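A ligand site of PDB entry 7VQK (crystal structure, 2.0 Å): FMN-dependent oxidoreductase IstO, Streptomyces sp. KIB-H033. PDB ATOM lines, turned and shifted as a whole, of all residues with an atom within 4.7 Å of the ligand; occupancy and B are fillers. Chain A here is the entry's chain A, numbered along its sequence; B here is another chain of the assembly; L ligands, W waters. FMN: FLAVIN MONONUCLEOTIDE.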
ATOM      1  N   ARG A  21     -27.535 -16.908 -11.316  1.00  0.00           N
ATOM      2  CA  ARG A  21     -26.809 -18.062 -11.812  1.00  0.00           C
ATOM      3  C   ARG A  21     -27.783 -19.031 -12.461  1.00  0.00           C
ATOM      4  O   ARG A  21     -28.992 -18.990 -12.214  1.00  0.00           O
ATOM      5  CB  ARG A  21     -26.068 -18.792 -10.669  1.00  0.00           C
ATOM      6  CG  ARG A  21     -25.059 -17.944  -9.928  1.00  0.00           C
ATOM      7  CD  ARG A  21     -23.911 -17.560 -10.847  1.00  0.00           C
ATOM      8  NE  ARG A  21     -23.396 -18.722 -11.564  1.00  0.00           N
ATOM      9  CZ  ARG A  21     -22.535 -19.588 -11.051  1.00  0.00           C
ATOM     10  NH1 ARG A  21     -22.059 -19.455  -9.822  1.00  0.00           N
ATOM     11  NH2 ARG A  21     -22.147 -20.636 -11.784  1.00  0.00           N
ATOM     12  N   THR A  22     -27.249 -19.915 -13.287  1.00  0.00           N
ATOM     13  CA  THR A  22     -28.046 -20.945 -13.932  1.00  0.00           C
ATOM     14  C   THR A  22     -28.227 -22.104 -12.956  1.00  0.00           C
ATOM     15  O   THR A  22     -27.229 -22.649 -12.454  1.00  0.00           O
ATOM     16  CB  THR A  22     -27.366 -21.404 -15.216  1.00  0.00           C
ATOM     17  OG1 THR A  22     -27.252 -20.293 -16.121  1.00  0.00           O
ATOM     18  CG2 THR A  22     -28.159 -22.511 -15.879  1.00  0.00           C
ATOM     19  N   ASN A  24     -28.933 -25.795 -11.654  1.00  0.00           N
ATOM     20  CA  ASN A  24     -28.878 -27.188 -12.080  1.00  0.00           C
ATOM     21  C   ASN A  24     -29.723 -28.098 -11.202  1.00  0.00           C
ATOM     22  O   ASN A  24     -29.880 -29.281 -11.536  1.00  0.00           O
ATOM     23  CB  ASN A  24     -27.432 -27.706 -12.087  1.00  0.00           C
ATOM     24  CG  ASN A  24     -26.552 -26.930 -13.059  1.00  0.00           C
ATOM     25  OD1 ASN A  24     -26.599 -27.146 -14.268  1.00  0.00           O
ATOM     26  ND2 ASN A  24     -25.759 -26.012 -12.520  1.00  0.00           N
ATOM     27  N   ASN A  77     -29.098 -34.161 -19.544  1.00  0.00           N
ATOM     28  CA  ASN A  77     -29.960 -33.073 -19.122  1.00  0.00           C
ATOM     29  C   ASN A  77     -31.252 -33.539 -18.458  1.00  0.00           C
ATOM     30  O   ASN A  77     -32.004 -32.712 -17.942  1.00  0.00           O
ATOM     31  CB  ASN A  77     -30.303 -32.186 -20.324  1.00  0.00           C
ATOM     32  CG  ASN A  77     -29.077 -31.493 -20.908  1.00  0.00           C
ATOM     33  OD1 ASN A  77     -28.197 -31.036 -20.166  1.00  0.00           O
ATOM     34  ND2 ASN A  77     -28.995 -31.451 -22.237  1.00  0.00           N
ATOM     35  N   LYS A  80     -31.908 -32.511 -14.624  1.00  0.00           N
ATOM     36  CA  LYS A  80     -32.383 -31.148 -14.419  1.00  0.00           C
ATOM     37  C   LYS A  80     -33.837 -30.994 -14.857  1.00  0.00           C
ATOM     38  O   LYS A  80     -34.669 -30.432 -14.133  1.00  0.00           O
ATOM     39  CB  LYS A  80     -31.494 -30.167 -15.191  1.00  0.00           C
ATOM     40  CG  LYS A  80     -30.018 -30.238 -14.813  1.00  0.00           C
ATOM     41  CD  LYS A  80     -29.119 -29.699 -15.938  1.00  0.00           C
ATOM     42  CE  LYS A  80     -27.714 -30.248 -15.810  1.00  0.00           C
ATOM     43  NZ  LYS A  80     -27.287 -30.996 -17.047  1.00  0.00           N
ATOM     44  N   LEU A 132     -36.055 -15.016 -25.621  1.00  0.00           N
ATOM     45  CA  LEU A 132     -35.555 -15.917 -24.592  1.00  0.00           C
ATOM     46  C   LEU A 132     -34.648 -15.172 -23.622  1.00  0.00           C
ATOM     47  O   LEU A 132     -34.704 -15.390 -22.402  1.00  0.00           O
ATOM     48  CB  LEU A 132     -34.800 -17.090 -25.226  1.00  0.00           C
ATOM     49  CG  LEU A 132     -33.950 -17.974 -24.277  1.00  0.00           C
ATOM     50  CD1 LEU A 132     -34.792 -18.596 -23.169  1.00  0.00           C
ATOM     51  CD2 LEU A 132     -33.217 -19.051 -25.053  1.00  0.00           C
ATOM     52  N   ARG A 140     -35.705 -14.333 -13.551  1.00  0.00           N
ATOM     53  CA  ARG A 140     -34.964 -13.807 -12.408  1.00  0.00           C
ATOM     54  C   ARG A 140     -35.702 -12.635 -11.770  1.00  0.00           C
ATOM     55  O   ARG A 140     -35.710 -12.492 -10.539  1.00  0.00           O
ATOM     56  CB  ARG A 140     -33.565 -13.407 -12.843  1.00  0.00           C
ATOM     57  CG  ARG A 140     -32.718 -14.607 -13.278  1.00  0.00           C
ATOM     58  CD  ARG A 140     -31.639 -14.183 -14.276  1.00  0.00           C
ATOM     59  NE  ARG A 140     -30.702 -15.274 -14.548  1.00  0.00           N
ATOM     60  CZ  ARG A 140     -29.470 -15.079 -15.012  1.00  0.00           C
ATOM     61  NH1 ARG A 140     -29.022 -13.862 -15.293  1.00  0.00           N
ATOM     62  NH2 ARG A 140     -28.655 -16.124 -15.159  1.00  0.00           N
ATOM     63  N   PRO A 148     -31.713 -22.817 -18.632  1.00  0.00           N
ATOM     64  CA  PRO A 148     -31.930 -23.067 -20.061  1.00  0.00           C
ATOM     65  C   PRO A 148     -31.263 -24.355 -20.498  1.00  0.00           C
ATOM     66  O   PRO A 148     -30.234 -24.768 -19.949  1.00  0.00           O
ATOM     67  CB  PRO A 148     -31.287 -21.847 -20.748  1.00  0.00           C
ATOM     68  CG  PRO A 148     -31.014 -20.847 -19.670  1.00  0.00           C
ATOM     69  CD  PRO A 148     -30.923 -21.609 -18.368  1.00  0.00           C
ATOM     70  N   ILE A 149     -31.862 -24.995 -21.498  1.00  0.00           N
ATOM     71  CA  ILE A 149     -31.419 -26.296 -21.969  1.00  0.00           C
ATOM     72  C   ILE A 149     -31.483 -26.326 -23.493  1.00  0.00           C
ATOM     73  O   ILE A 149     -32.553 -26.081 -24.074  1.00  0.00           O
ATOM     74  CB  ILE A 149     -32.268 -27.440 -21.380  1.00  0.00           C
ATOM     75  CG1 ILE A 149     -32.067 -27.558 -19.861  1.00  0.00           C
ATOM     76  CG2 ILE A 149     -31.992 -28.744 -22.127  1.00  0.00           C
ATOM     77  CD1 ILE A 149     -30.707 -28.093 -19.443  1.00  0.00           C
ATOM     78  N   ALA A 150     -30.362 -26.635 -24.148  1.00  0.00           N
ATOM     79  CA  ALA A 150     -30.331 -26.805 -25.587  1.00  0.00           C
ATOM     80  C   ALA A 150     -30.120 -28.253 -26.019  1.00  0.00           C
ATOM     81  O   ALA A 150     -30.374 -28.587 -27.189  1.00  0.00           O
ATOM     82  CB  ALA A 150     -29.235 -25.925 -26.216  1.00  0.00           C
ATOM     83  N   GLY A 151     -29.700 -29.124 -25.114  1.00  0.00           N
ATOM     84  CA  GLY A 151     -29.458 -30.522 -25.458  1.00  0.00           C
ATOM     85  C   GLY A 151     -30.714 -31.361 -25.498  1.00  0.00           C
ATOM     86  O   GLY A 151     -30.982 -32.127 -24.560  1.00  0.00           O
ATOM     87  N   ARG A 186     -18.711 -19.780 -10.834  1.00  0.00           N
ATOM     88  CA  ARG A 186     -18.892 -18.983 -12.038  1.00  0.00           C
ATOM     89  C   ARG A 186     -17.745 -19.234 -12.998  1.00  0.00           C
ATOM     90  O   ARG A 186     -16.582 -19.317 -12.588  1.00  0.00           O
ATOM     91  CB  ARG A 186     -18.959 -17.493 -11.679  1.00  0.00           C
ATOM     92  CG  ARG A 186     -19.331 -16.567 -12.834  1.00  0.00           C
ATOM     93  CD  ARG A 186     -20.859 -16.596 -13.128  1.00  0.00           C
ATOM     94  NE  ARG A 186     -21.582 -15.542 -12.418  1.00  0.00           N
ATOM     95  CZ  ARG A 186     -22.856 -15.233 -12.645  1.00  0.00           C
ATOM     96  NH1 ARG A 186     -23.573 -15.890 -13.538  1.00  0.00           N
ATOM     97  NH2 ARG A 186     -23.412 -14.239 -11.961  1.00  0.00           N
ATOM     98  N   LEU A 187     -18.056 -19.370 -14.265  1.00  0.00           N
ATOM     99  CA  LEU A 187     -17.033 -19.584 -15.276  1.00  0.00           C
ATOM    100  C   LEU A 187     -16.530 -18.256 -15.810  1.00  0.00           C
ATOM    101  O   LEU A 187     -17.102 -17.196 -15.543  1.00  0.00           O
ATOM    102  CB  LEU A 187     -17.590 -20.456 -16.402  1.00  0.00           C
ATOM    103  CG  LEU A 187     -18.011 -21.856 -15.933  1.00  0.00           C
ATOM    104  CD1 LEU A 187     -18.662 -22.629 -17.066  1.00  0.00           C
ATOM    105  CD2 LEU A 187     -16.786 -22.614 -15.398  1.00  0.00           C
ATOM    106  N   ARG A 189     -15.586 -15.027 -18.206  1.00  0.00           N
ATOM    107  CA  ARG A 189     -16.209 -14.240 -19.251  1.00  0.00           C
ATOM    108  C   ARG A 189     -15.092 -13.527 -20.010  1.00  0.00           C
ATOM    109  O   ARG A 189     -14.088 -13.137 -19.406  1.00  0.00           O
ATOM    110  CB  ARG A 189     -17.203 -13.222 -18.666  1.00  0.00           C
ATOM    111  CG  ARG A 189     -18.412 -13.835 -17.914  1.00  0.00           C
ATOM    112  CD  ARG A 189     -19.238 -14.792 -18.790  1.00  0.00           C
ATOM    113  NE  ARG A 189     -20.554 -15.087 -18.233  1.00  0.00           N
ATOM    114  CZ  ARG A 189     -20.820 -16.101 -17.406  1.00  0.00           C
ATOM    115  NH1 ARG A 189     -19.864 -16.911 -16.979  1.00  0.00           N
ATOM    116  NH2 ARG A 189     -22.072 -16.293 -16.998  1.00  0.00           N
ATOM    117  N   TRP B  45     -22.595 -11.256 -17.856  1.00  0.00           N
ATOM    118  CA  TRP B  45     -22.951 -12.393 -17.008  1.00  0.00           C
ATOM    119  C   TRP B  45     -24.136 -13.180 -17.550  1.00  0.00           C
ATOM    120  O   TRP B  45     -24.283 -14.361 -17.234  1.00  0.00           O
ATOM    121  CB  TRP B  45     -23.210 -11.899 -15.578  1.00  0.00           C
ATOM    122  CG  TRP B  45     -21.951 -11.318 -15.029  1.00  0.00           C
ATOM    123  CD1 TRP B  45     -21.691 -10.009 -14.764  1.00  0.00           C
ATOM    124  CD2 TRP B  45     -20.744 -12.035 -14.762  1.00  0.00           C
ATOM    125  NE1 TRP B  45     -20.397  -9.866 -14.319  1.00  0.00           N
ATOM    126  CE2 TRP B  45     -19.795 -11.094 -14.316  1.00  0.00           C
ATOM    127  CE3 TRP B  45     -20.373 -13.380 -14.840  1.00  0.00           C
ATOM    128  CZ2 TRP B  45     -18.501 -11.456 -13.961  1.00  0.00           C
ATOM    129  CZ3 TRP B  45     -19.083 -13.734 -14.490  1.00  0.00           C
ATOM    130  CH2 TRP B  45     -18.156 -12.771 -14.053  1.00  0.00           C
ATOM    131  N   PRO B  47     -26.471 -15.574 -19.422  1.00  0.00           N
ATOM    132  CA  PRO B  47     -25.976 -16.901 -19.818  1.00  0.00           C
ATOM    133  C   PRO B  47     -26.131 -17.204 -21.303  1.00  0.00           C
ATOM    134  O   PRO B  47     -27.083 -16.789 -21.963  1.00  0.00           O
ATOM    135  CB  PRO B  47     -26.853 -17.857 -18.999  1.00  0.00           C
ATOM    136  CG  PRO B  47     -28.163 -17.087 -18.840  1.00  0.00           C
ATOM    137  CD  PRO B  47     -27.752 -15.640 -18.694  1.00  0.00           C
ATOM    138  N   THR B  48     -25.158 -17.972 -21.815  1.00  0.00           N
ATOM    139  CA  THR B  48     -25.206 -18.541 -23.149  1.00  0.00           C
ATOM    140  C   THR B  48     -24.890 -20.031 -23.087  1.00  0.00           C
ATOM    141  O   THR B  48     -24.284 -20.522 -22.130  1.00  0.00           O
ATOM    142  CB  THR B  48     -24.225 -17.823 -24.099  1.00  0.00           C
ATOM    143  OG1 THR B  48     -22.941 -17.735 -23.484  1.00  0.00           O
ATOM    144  CG2 THR B  48     -24.743 -16.414 -24.422  1.00  0.00           C
ATOM    145  N   SER B  49     -25.289 -20.736 -24.150  1.00  0.00           N
ATOM    146  CA  SER B  49     -25.065 -22.181 -24.241  1.00  0.00           C
ATOM    147  C   SER B  49     -23.581 -22.531 -24.110  1.00  0.00           C
ATOM    148  O   SER B  49     -22.752 -22.014 -24.853  1.00  0.00           O
ATOM    149  CB  SER B  49     -25.577 -22.704 -25.577  1.00  0.00           C
ATOM    150  OG  SER B  49     -25.327 -24.097 -25.695  1.00  0.00           O
ATOM    151  N   MET B  50     -23.270 -23.426 -23.180  1.00  0.00           N
ATOM    152  CA  MET B  50     -21.877 -23.795 -22.910  1.00  0.00           C
ATOM    153  C   MET B  50     -20.974 -22.584 -22.667  1.00  0.00           C
ATOM    154  O   MET B  50     -19.777 -22.622 -22.960  1.00  0.00           O
ATOM    155  CB  MET B  50     -21.286 -24.618 -24.067  1.00  0.00           C
ATOM    156  CG  MET B  50     -21.854 -26.034 -24.162  1.00  0.00           C
ATOM    157  SD  MET B  50     -20.984 -27.107 -25.554  1.00  0.00           S
ATOM    158  CE  MET B  50     -22.291 -28.543 -25.674  1.00  0.00           C
ATOM    159  N   ASN B  51     -21.557 -21.501 -22.148  1.00  0.00           N
ATOM    160  CA  ASN B  51     -20.810 -20.274 -21.856  1.00  0.00           C
ATOM    161  C   ASN B  51     -20.067 -19.772 -23.092  1.00  0.00           C
ATOM    162  O   ASN B  51     -18.998 -19.166 -22.983  1.00  0.00           O
ATOM    163  CB  ASN B  51     -19.838 -20.507 -20.690  1.00  0.00           C
ATOM    164  CG  ASN B  51     -19.341 -19.210 -20.052  1.00  0.00           C
ATOM    165  OD1 ASN B  51     -20.082 -18.234 -19.916  1.00  0.00           O
ATOM    166  ND2 ASN B  51     -18.079 -19.222 -19.627  1.00  0.00           N
ATOM    167  N   PHE B 104     -15.326 -22.891 -21.134  1.00  0.00           N
ATOM    168  CA  PHE B 104     -16.109 -24.028 -20.638  1.00  0.00           C
ATOM    169  C   PHE B 104     -15.145 -25.149 -20.304  1.00  0.00           C
ATOM    170  O   PHE B 104     -15.179 -26.226 -20.903  1.00  0.00           O
ATOM    171  CB  PHE B 104     -17.149 -24.472 -21.661  1.00  0.00           C
ATOM    172  CG  PHE B 104     -18.393 -25.090 -21.047  1.00  0.00           C
ATOM    173  CD1 PHE B 104     -19.166 -24.392 -20.132  1.00  0.00           C
ATOM    174  CD2 PHE B 104     -18.778 -26.388 -21.381  1.00  0.00           C
ATOM    175  CE1 PHE B 104     -20.289 -24.955 -19.571  1.00  0.00           C
ATOM    176  CE2 PHE B 104     -19.909 -26.966 -20.814  1.00  0.00           C
ATOM    177  CZ  PHE B 104     -20.667 -26.239 -19.911  1.00  0.00           C
ATOM    178  N   PHE B 126     -27.674 -17.857 -32.704  1.00  0.00           N
ATOM    179  CA  PHE B 126     -28.681 -17.944 -31.653  1.00  0.00           C
ATOM    180  C   PHE B 126     -28.182 -17.320 -30.355  1.00  0.00           C
ATOM    181  O   PHE B 126     -28.882 -16.530 -29.719  1.00  0.00           O
ATOM    182  CB  PHE B 126     -29.082 -19.410 -31.446  1.00  0.00           C
ATOM    183  CG  PHE B 126     -30.215 -19.609 -30.445  1.00  0.00           C
ATOM    184  CD1 PHE B 126     -29.950 -19.791 -29.104  1.00  0.00           C
ATOM    185  CD2 PHE B 126     -31.534 -19.611 -30.877  1.00  0.00           C
ATOM    186  CE1 PHE B 126     -30.983 -19.968 -28.185  1.00  0.00           C
ATOM    187  CE2 PHE B 126     -32.576 -19.801 -29.969  1.00  0.00           C
ATOM    188  CZ  PHE B 126     -32.299 -19.976 -28.629  1.00  0.00           C
ATOM    189  N   ASN B 127     -26.948 -17.672 -29.930  1.00  0.00           N
ATOM    190  CA  ASN B 127     -26.444 -17.129 -28.679  1.00  0.00           C
ATOM    191  C   ASN B 127     -26.044 -15.669 -28.810  1.00  0.00           C
ATOM    192  O   ASN B 127     -26.115 -14.928 -27.820  1.00  0.00           O
ATOM    193  CB  ASN B 127     -25.269 -17.984 -28.181  1.00  0.00           C
ATOM    194  CG  ASN B 127     -25.751 -19.284 -27.543  1.00  0.00           C
ATOM    195  OD1 ASN B 127     -26.070 -19.340 -26.357  1.00  0.00           O
ATOM    196  ND2 ASN B 127     -25.836 -20.345 -28.357  1.00  0.00           N
ATOM    197  N   LEU B 130     -29.372 -14.004 -28.266  1.00  0.00           N
ATOM    198  CA  LEU B 130     -29.543 -13.999 -26.821  1.00  0.00           C
ATOM    199  C   LEU B 130     -28.786 -12.848 -26.181  1.00  0.00           C
ATOM    200  O   LEU B 130     -29.335 -12.091 -25.369  1.00  0.00           O
ATOM    201  CB  LEU B 130     -29.078 -15.347 -26.274  1.00  0.00           C
ATOM    202  CG  LEU B 130     -29.494 -15.863 -24.916  1.00  0.00           C
ATOM    203  CD1 LEU B 130     -31.018 -15.811 -24.763  1.00  0.00           C
ATOM    204  CD2 LEU B 130     -28.976 -17.290 -24.827  1.00  0.00           C
HETATM  205  N1  FMN L   1     -26.649 -26.443 -19.459  1.00  0.00           N
HETATM  206  C2  FMN L   1     -26.672 -27.815 -19.511  1.00  0.00           C
HETATM  207  O2  FMN L   1     -26.233 -28.456 -18.562  1.00  0.00           O
HETATM  208  N3  FMN L   1     -27.194 -28.455 -20.605  1.00  0.00           N
HETATM  209  C4  FMN L   1     -27.689 -27.730 -21.659  1.00  0.00           C
HETATM  210  O4  FMN L   1     -28.148 -28.329 -22.628  1.00  0.00           O
HETATM  211  C4A FMN L   1     -27.668 -26.328 -21.622  1.00  0.00           C
HETATM  212  N5  FMN L   1     -28.151 -25.581 -22.676  1.00  0.00           N
HETATM  213  C5A FMN L   1     -28.134 -24.197 -22.600  1.00  0.00           C
HETATM  214  C6  FMN L   1     -28.642 -23.422 -23.649  1.00  0.00           C
HETATM  215  C7  FMN L   1     -28.609 -22.037 -23.586  1.00  0.00           C
HETATM  216  C7M FMN L   1     -29.180 -21.234 -24.738  1.00  0.00           C
HETATM  217  C8  FMN L   1     -28.094 -21.398 -22.468  1.00  0.00           C
HETATM  218  C8M FMN L   1     -28.055 -19.910 -22.357  1.00  0.00           C
HETATM  219  C9  FMN L   1     -27.598 -22.166 -21.417  1.00  0.00           C
HETATM  220  C9A FMN L   1     -27.606 -23.566 -21.484  1.00  0.00           C
HETATM  221  N10 FMN L   1     -27.086 -24.319 -20.433  1.00  0.00           N
HETATM  222  C10 FMN L   1     -27.132 -25.696 -20.513  1.00  0.00           C
HETATM  223  C1' FMN L   1     -26.525 -23.652 -19.213  1.00  0.00           C
HETATM  224  C2' FMN L   1     -25.195 -22.946 -19.486  1.00  0.00           C
HETATM  225  O2' FMN L   1     -24.125 -23.866 -19.460  1.00  0.00           O
HETATM  226  C3' FMN L   1     -24.927 -21.881 -18.409  1.00  0.00           C
HETATM  227  O3' FMN L   1     -25.984 -20.941 -18.417  1.00  0.00           O
HETATM  228  C4' FMN L   1     -23.636 -21.103 -18.597  1.00  0.00           C
HETATM  229  O4' FMN L   1     -22.550 -21.985 -18.425  1.00  0.00           O
HETATM  230  C5' FMN L   1     -23.432 -19.954 -17.619  1.00  0.00           C
HETATM  231  O5' FMN L   1     -23.652 -20.373 -16.300  1.00  0.00           O
HETATM  232  P   FMN L   1     -24.095 -19.275 -15.193  1.00  0.00           P
HETATM  233  O1P FMN L   1     -23.067 -18.188 -15.092  1.00  0.00           O
HETATM  234  O2P FMN L   1     -24.249 -19.985 -13.866  1.00  0.00           O
HETATM  235  O3P FMN L   1     -25.407 -18.668 -15.610  1.00  0.00           O
HETATM  236  O   HOH W   1     -26.971 -26.049 -16.497  1.00  0.00           O
HETATM  237  O   HOH W   2     -25.715 -26.445 -24.584  1.00  0.00           O
HETATM  238  O   HOH W   3     -20.636 -19.403 -15.497  1.00  0.00           O
HETATM  239  O   HOH W   4     -24.214 -25.823 -21.676  1.00  0.00           O
HETATM  240  O   HOH W   5     -25.822 -16.010 -15.751  1.00  0.00           O
HETATM  241  O   HOH W   6     -24.200 -22.401 -13.501  1.00  0.00           O
HETATM  242  O   HOH W   7     -26.457 -30.861 -23.448  1.00  0.00           O
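The backbone NH (N) of Gly 151 lies within hydrogen-bond range of an oxygen (O4) of the ligand. An oxygen (O3P) of the ligand sits at hydrogen-bond distance from the side-chain hydroxyl (OG1) of Thr 22, 2.5 Å away. An oxygen (O2P) of the ligand is in salt-bridge range of the guanidinium group of Arg 21, 2.8 Å away. N of Thr 22 sits at hydrogen-bond distance from O2P of the ligand, at 3.1 Å. An oxygen (O1P) of the ligand lies within salt-bridge range of the guanidinium group (NH2) of Arg 189, at 2.9 Å. NZ of Lys 80 sits at hydrogen-bond distance from O2 of the ligand. OD1 of Asn 77 is in hydrogen-bond range of N3 of the ligand. The guanidinium group (NH1) of Arg 186 lies within salt-bridge range of an oxygen (O1P) of the ligand. A nitrogen (N5) of the ligand lies within hydrogen-bond range of the backbone NH of Ala 150, at 2.9 Å.
The side-chain amino group of Lys 80 lies within hydrogen-bond range of the side-chain amide oxygen of Asn 77, at 3.2 Å. The backbone NH of Ser 49 of chain B lies within hydrogen-bond range of the side-chain amide oxygen of Asn 127 of chain B (2.7 Å). The guanidinium group (NH1) of Arg 189 lies within hydrogen-bond range of the side-chain amide oxygen (OD1) of Asn 51 of chain B (3.2 Å). NH1 of Arg 189 lies within hydrogen-bond range of O of Leu 187 (3.1 Å). ND2 of Asn 77 is in hydrogen-bond range of O of Gly 151, 3.1 Å away. The backbone carbonyl oxygen (O) of Trp 45 of chain B lies within hydrogen-bond range of the guanidinium group (NH2) of Arg 189, at 2.9 Å.
The backbone carbonyl oxygen (O) of Pro 148 lies close to a nitrogen (N10) of the ligand (3.2 Å). Residues that only touch the ligand: Thr 48 of chain B (3.3 Å), Pro 47 of chain B (3.3 Å), Ser 49 of chain B (3.3 Å), Ile 149 (3.4 Å), Leu 130 of chain B (3.7 Å), Asn 51 of chain B (3.8 Å), Met 50 of chain B (3.8 Å), Phe 104 of chain B (3.9 Å) and Asn 127 of chain B (3.99 Å). Hydrophobic or aromatic side chains that line the ligand: Pro 148, Ile 149, Ala 150, Pro 47 of chain B, Phe 104 of chain B and Leu 130 of chain B. Along chain A the residues within 4 Å of the ligand span positions 21 to 189. The nearest printed residue that does not touch the ligand is Phe 126 of chain B (4.1 Å).
Water W6 lies within hydrogen-bond range of O2P of the ligand (2.4 Å), NH2 of Arg 21 (3.2 Å) and O of Thr 22 (3.2 Å). Water W5 lies within hydrogen-bond range of O3P of the ligand (2.7 Å), O of Trp 45 of chain B (2.7 Å), NH2 of Arg 140 (2.9 Å) and NH1 of Arg 186 (3.2 Å). Water W4 bridges O2' of the ligand (3.0 Å) and N of Met 50 of chain B (3.0 Å). Water W1 bridges OD1 of Asn 24 (2.5 Å) and N1 of the ligand (3.0 Å). Water W7 lies within hydrogen-bond range of the side-chain amide nitrogen of Asn 77 and an oxygen (O4) of the ligand. Water W2 bridges OG of Ser 49 of chain B and N5 of the ligand.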
